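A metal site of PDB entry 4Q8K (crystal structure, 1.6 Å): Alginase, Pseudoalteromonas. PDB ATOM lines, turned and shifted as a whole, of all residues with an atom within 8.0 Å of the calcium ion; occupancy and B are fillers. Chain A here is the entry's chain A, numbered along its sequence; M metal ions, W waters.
The backbone carbonyl oxygen of Thr 243 lies close to the backbone NH of Val 252. N of Gly 256 lies within hydrogen-bond range of OD2 of Asp 242 (2.9 Å). O of Asp 242 lies within hydrogen-bond range of N of Asn 254. N of Gly 219 is in hydrogen-bond range of OD2 of Asp 242 (2.7 Å). The backbone NH of Asp 242 is in hydrogen-bond range of the backbone carbonyl oxygen of Gly 220 (2.9 Å). The side-chain carboxylate (OD1) of Asp 259 lies within hydrogen-bond range of the backbone NH (N) of Asp 250, at 2.8 Å.
Of the 21 residues printed, 5 come within 4 Å of the calcium ion.
OD1 of Asp 242 is bound to the calcium ion. The calcium ion is bound by O of Val 252 (2.4 Å). The calcium ion is bound by O of Ile 257 (2.4 Å). The calcium ion is bound by OD1 of Asn 255, at 2.4 Å. OD2 of Asp 250 binds the calcium ion, 2.5 Å away. Water W1 binds the calcium ion. The calcium ion has six donor atoms within binding distance.
Water W1 lies within hydrogen-bond range of OD2 of Asp 259 (2.6 Å), O of Thr 243 (2.8 Å) and N of Val 252 (3.4 Å).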
ATOM      1  N   ASP A 218     -11.444  -3.568 -17.100  1.00  0.00           N
ATOM      2  CA  ASP A 218     -10.210  -2.834 -17.307  1.00  0.00           C
ATOM      3  C   ASP A 218      -9.038  -3.541 -16.626  1.00  0.00           C
ATOM      4  O   ASP A 218      -9.145  -4.014 -15.488  1.00  0.00           O
ATOM      5  CB  ASP A 218     -10.314  -1.395 -16.764  1.00  0.00           C
ATOM      6  CG  ASP A 218     -11.338  -0.551 -17.528  1.00  0.00           C
ATOM      7  OD1 ASP A 218     -11.872  -1.001 -18.553  1.00  0.00           O
ATOM      8  OD2 ASP A 218     -11.614   0.583 -17.084  1.00  0.00           O
ATOM      9  N   GLY A 219      -7.919  -3.635 -17.342  1.00  0.00           N
ATOM     10  CA  GLY A 219      -6.691  -4.182 -16.803  1.00  0.00           C
ATOM     11  C   GLY A 219      -6.554  -5.686 -16.993  1.00  0.00           C
ATOM     12  O   GLY A 219      -5.515  -6.266 -16.703  1.00  0.00           O
ATOM     13  N   GLY A 220      -7.616  -6.317 -17.492  1.00  0.00           N
ATOM     14  CA  GLY A 220      -7.602  -7.757 -17.697  1.00  0.00           C
ATOM     15  C   GLY A 220      -6.599  -8.187 -18.756  1.00  0.00           C
ATOM     16  O   GLY A 220      -6.276  -7.420 -19.683  1.00  0.00           O
ATOM     17  N   SER A 241      -5.178  -8.047 -23.957  1.00  0.00           N
ATOM     18  CA  SER A 241      -4.359  -7.580 -22.836  1.00  0.00           C
ATOM     19  C   SER A 241      -4.462  -6.069 -22.617  1.00  0.00           C
ATOM     20  O   SER A 241      -4.311  -5.291 -23.544  1.00  0.00           O
ATOM     21  CB  SER A 241      -2.897  -7.958 -23.104  1.00  0.00           C
ATOM     22  OG  SER A 241      -2.012  -7.425 -22.137  1.00  0.00           O
ATOM     23  N   ASP A 242      -4.676  -5.670 -21.357  1.00  0.00           N
ATOM     24  CA  ASP A 242      -4.851  -4.255 -21.035  1.00  0.00           C
ATOM     25  C   ASP A 242      -3.746  -3.815 -20.082  1.00  0.00           C
ATOM     26  O   ASP A 242      -4.015  -3.318 -18.993  1.00  0.00           O
ATOM     27  CB  ASP A 242      -6.245  -3.999 -20.433  1.00  0.00           C
ATOM     28  CG  ASP A 242      -6.552  -2.516 -20.245  1.00  0.00           C
ATOM     29  OD1 ASP A 242      -5.810  -1.681 -20.798  1.00  0.00           O
ATOM     30  OD2 ASP A 242      -7.536  -2.168 -19.555  1.00  0.00           O
ATOM     31  N   THR A 243      -2.491  -4.002 -20.482  1.00  0.00           N
ATOM     32  CA  THR A 243      -1.344  -3.712 -19.618  1.00  0.00           C
ATOM     33  C   THR A 243      -0.457  -2.601 -20.157  1.00  0.00           C
ATOM     34  O   THR A 243      -0.693  -2.065 -21.246  1.00  0.00           O
ATOM     35  CB  THR A 243      -0.430  -4.940 -19.446  1.00  0.00           C
ATOM     36  OG1 THR A 243       0.339  -5.121 -20.636  1.00  0.00           O
ATOM     37  CG2 THR A 243      -1.237  -6.195 -19.134  1.00  0.00           C
ATOM     38  N   ASP A 244       0.596  -2.300 -19.398  1.00  0.00           N
ATOM     39  CA  ASP A 244       1.567  -1.282 -19.774  1.00  0.00           C
ATOM     40  C   ASP A 244       2.752  -1.878 -20.519  1.00  0.00           C
ATOM     41  O   ASP A 244       3.765  -1.207 -20.723  1.00  0.00           O
ATOM     42  CB  ASP A 244       2.081  -0.555 -18.527  1.00  0.00           C
ATOM     43  CG  ASP A 244       1.637   0.900 -18.458  1.00  0.00           C
ATOM     44  OD1 ASP A 244       0.880   1.346 -19.343  1.00  0.00           O
ATOM     45  OD2 ASP A 244       2.036   1.593 -17.490  1.00  0.00           O
ATOM     46  N   ASN A 249      -0.077  -1.343 -30.024  1.00  0.00           N
ATOM     47  CA  ASN A 249      -0.794  -0.149 -30.491  1.00  0.00           C
ATOM     48  C   ASN A 249      -1.250   0.775 -29.372  1.00  0.00           C
ATOM     49  O   ASN A 249      -1.234   2.004 -29.527  1.00  0.00           O
ATOM     50  CB  ASN A 249      -2.011  -0.519 -31.340  1.00  0.00           C
ATOM     51  CG  ASN A 249      -1.645  -1.197 -32.649  1.00  0.00           C
ATOM     52  OD1 ASN A 249      -0.485  -1.456 -32.934  1.00  0.00           O
ATOM     53  ND2 ASN A 249      -2.663  -1.489 -33.446  1.00  0.00           N
ATOM     54  N   ASP A 250      -1.689   0.188 -28.258  1.00  0.00           N
ATOM     55  CA  ASP A 250      -2.120   0.963 -27.102  1.00  0.00           C
ATOM     56  C   ASP A 250      -1.033   0.945 -26.027  1.00  0.00           C
ATOM     57  O   ASP A 250      -0.389   1.966 -25.782  1.00  0.00           O
ATOM     58  CB  ASP A 250      -3.452   0.428 -26.549  1.00  0.00           C
ATOM     59  CG  ASP A 250      -4.014   1.274 -25.435  1.00  0.00           C
ATOM     60  OD1 ASP A 250      -4.735   2.256 -25.712  1.00  0.00           O
ATOM     61  OD2 ASP A 250      -3.748   0.955 -24.259  1.00  0.00           O
ATOM     62  N   SER A 251      -0.815  -0.224 -25.439  1.00  0.00           N
ATOM     63  CA  SER A 251       0.239  -0.419 -24.438  1.00  0.00           C
ATOM     64  C   SER A 251       0.048   0.496 -23.225  1.00  0.00           C
ATOM     65  O   SER A 251       1.006   0.823 -22.539  1.00  0.00           O
ATOM     66  CB  SER A 251       1.623  -0.199 -25.051  1.00  0.00           C
ATOM     67  OG  SER A 251       1.991  -1.280 -25.896  1.00  0.00           O
ATOM     68  N   VAL A 252      -1.195   0.885 -22.966  1.00  0.00           N
ATOM     69  CA  VAL A 252      -1.495   1.688 -21.795  1.00  0.00           C
ATOM     70  C   VAL A 252      -2.281   0.869 -20.777  1.00  0.00           C
ATOM     71  O   VAL A 252      -3.382   0.434 -21.047  1.00  0.00           O
ATOM     72  CB  VAL A 252      -2.300   2.956 -22.156  1.00  0.00           C
ATOM     73  CG1 VAL A 252      -2.714   3.687 -20.902  1.00  0.00           C
ATOM     74  CG2 VAL A 252      -1.487   3.864 -23.075  1.00  0.00           C
ATOM     75  N   ALA A 253      -1.705   0.673 -19.599  1.00  0.00           N
ATOM     76  CA  ALA A 253      -2.331  -0.173 -18.588  1.00  0.00           C
ATOM     77  C   ALA A 253      -3.703   0.327 -18.141  1.00  0.00           C
ATOM     78  O   ALA A 253      -3.887   1.520 -17.905  1.00  0.00           O
ATOM     79  CB  ALA A 253      -1.417  -0.340 -17.388  1.00  0.00           C
ATOM     80  N   ASN A 254      -4.654  -0.601 -18.044  1.00  0.00           N
ATOM     81  CA  ASN A 254      -5.878  -0.352 -17.295  1.00  0.00           C
ATOM     82  C   ASN A 254      -6.764   0.773 -17.844  1.00  0.00           C
ATOM     83  O   ASN A 254      -7.447   1.451 -17.065  1.00  0.00           O
ATOM     84  CB  ASN A 254      -5.525  -0.069 -15.821  1.00  0.00           C
ATOM     85  CG  ASN A 254      -6.684  -0.301 -14.874  1.00  0.00           C
ATOM     86  OD1 ASN A 254      -7.513  -1.191 -15.084  1.00  0.00           O
ATOM     87  ND2 ASN A 254      -6.754   0.507 -13.808  1.00  0.00           N
ATOM     88  N   ASN A 255      -6.787   0.958 -19.171  1.00  0.00           N
ATOM     89  CA  ASN A 255      -7.618   2.005 -19.764  1.00  0.00           C
ATOM     90  C   ASN A 255      -8.801   1.474 -20.582  1.00  0.00           C
ATOM     91  O   ASN A 255      -9.507   2.241 -21.239  1.00  0.00           O
ATOM     92  CB  ASN A 255      -6.795   2.977 -20.594  1.00  0.00           C
ATOM     93  CG  ASN A 255      -6.373   2.395 -21.925  1.00  0.00           C
ATOM     94  OD1 ASN A 255      -6.398   1.189 -22.102  1.00  0.00           O
ATOM     95  ND2 ASN A 255      -5.986   3.254 -22.869  1.00  0.00           N
ATOM     96  N   GLY A 256      -9.008   0.157 -20.546  1.00  0.00           N
ATOM     97  CA  GLY A 256     -10.167  -0.432 -21.196  1.00  0.00           C
ATOM     98  C   GLY A 256      -9.922  -0.737 -22.661  1.00  0.00           C
ATOM     99  O   GLY A 256     -10.758  -1.360 -23.324  1.00  0.00           O
ATOM    100  N   ILE A 257      -8.786  -0.285 -23.187  1.00  0.00           N
ATOM    101  CA  ILE A 257      -8.422  -0.593 -24.566  1.00  0.00           C
ATOM    102  C   ILE A 257      -7.471  -1.779 -24.553  1.00  0.00           C
ATOM    103  O   ILE A 257      -6.334  -1.674 -24.136  1.00  0.00           O
ATOM    104  CB  ILE A 257      -7.751   0.602 -25.270  1.00  0.00           C
ATOM    105  CG1 ILE A 257      -8.708   1.800 -25.286  1.00  0.00           C
ATOM    106  CG2 ILE A 257      -7.330   0.225 -26.691  1.00  0.00           C
ATOM    107  CD1 ILE A 257      -8.122   3.040 -25.953  1.00  0.00           C
ATOM    108  N   PHE A 258      -7.960  -2.934 -25.007  1.00  0.00           N
ATOM    109  CA  PHE A 258      -7.146  -4.134 -24.966  1.00  0.00           C
ATOM    110  C   PHE A 258      -6.308  -4.255 -26.229  1.00  0.00           C
ATOM    111  O   PHE A 258      -6.822  -4.109 -27.332  1.00  0.00           O
ATOM    112  CB  PHE A 258      -8.037  -5.368 -24.822  1.00  0.00           C
ATOM    113  CG  PHE A 258      -8.859  -5.354 -23.568  1.00  0.00           C
ATOM    114  CD1 PHE A 258     -10.107  -4.751 -23.548  1.00  0.00           C
ATOM    115  CD2 PHE A 258      -8.353  -5.899 -22.393  1.00  0.00           C
ATOM    116  CE1 PHE A 258     -10.858  -4.727 -22.380  1.00  0.00           C
ATOM    117  CE2 PHE A 258      -9.102  -5.865 -21.223  1.00  0.00           C
ATOM    118  CZ  PHE A 258     -10.357  -5.269 -21.218  1.00  0.00           C
ATOM    119  N   ASP A 259      -5.013  -4.497 -26.056  1.00  0.00           N
ATOM    120  CA  ASP A 259      -4.149  -4.854 -27.161  1.00  0.00           C
ATOM    121  C   ASP A 259      -4.399  -6.318 -27.507  1.00  0.00           C
ATOM    122  O   ASP A 259      -4.538  -7.163 -26.624  1.00  0.00           O
ATOM    123  CB  ASP A 259      -2.687  -4.678 -26.760  1.00  0.00           C
ATOM    124  CG  ASP A 259      -2.306  -3.224 -26.583  1.00  0.00           C
ATOM    125  OD1 ASP A 259      -2.377  -2.483 -27.584  1.00  0.00           O
ATOM    126  OD2 ASP A 259      -1.969  -2.828 -25.462  1.00  0.00           O
ATOM    127  N   THR A 278      -6.477  -3.491 -31.578  1.00  0.00           N
ATOM    128  CA  THR A 278      -6.994  -3.113 -30.265  1.00  0.00           C
ATOM    129  C   THR A 278      -8.516  -3.222 -30.274  1.00  0.00           C
ATOM    130  O   THR A 278      -9.147  -3.182 -31.332  1.00  0.00           O
ATOM    131  CB  THR A 278      -6.623  -1.663 -29.889  1.00  0.00           C
ATOM    132  OG1 THR A 278      -7.138  -0.764 -30.878  1.00  0.00           O
ATOM    133  CG2 THR A 278      -5.114  -1.497 -29.770  1.00  0.00           C
ATOM    134  N   MET A 279      -9.101  -3.369 -29.085  1.00  0.00           N
ATOM    135  CA  MET A 279     -10.544  -3.460 -28.961  1.00  0.00           C
ATOM    136  C   MET A 279     -10.978  -2.965 -27.597  1.00  0.00           C
ATOM    137  O   MET A 279     -10.182  -2.949 -26.663  1.00  0.00           O
ATOM    138  CB  MET A 279     -11.017  -4.916 -29.119  1.00  0.00           C
ATOM    139  CG  MET A 279     -10.479  -5.859 -28.041  1.00  0.00           C
ATOM    140  SD  MET A 279     -10.847  -7.598 -28.387  1.00  0.00           S
ATOM    141  CE  MET A 279     -12.627  -7.512 -28.658  1.00  0.00           C
ATOM    142  N   PRO A 328      -1.475  -5.126 -14.207  1.00  0.00           N
ATOM    143  CA  PRO A 328      -1.321  -4.534 -15.540  1.00  0.00           C
ATOM    144  C   PRO A 328      -0.330  -3.365 -15.578  1.00  0.00           C
ATOM    145  O   PRO A 328       0.202  -3.061 -16.649  1.00  0.00           O
ATOM    146  CB  PRO A 328      -2.737  -4.063 -15.877  1.00  0.00           C
ATOM    147  CG  PRO A 328      -3.349  -3.791 -14.542  1.00  0.00           C
ATOM    148  CD  PRO A 328      -2.801  -4.860 -13.636  1.00  0.00           C
HETATM  149 CA    CA M   1      -4.829  -0.564 -22.646  1.00  0.00          CA
HETATM  150  O   HOH W   1      -2.862  -2.067 -23.089  1.00  0.00           O
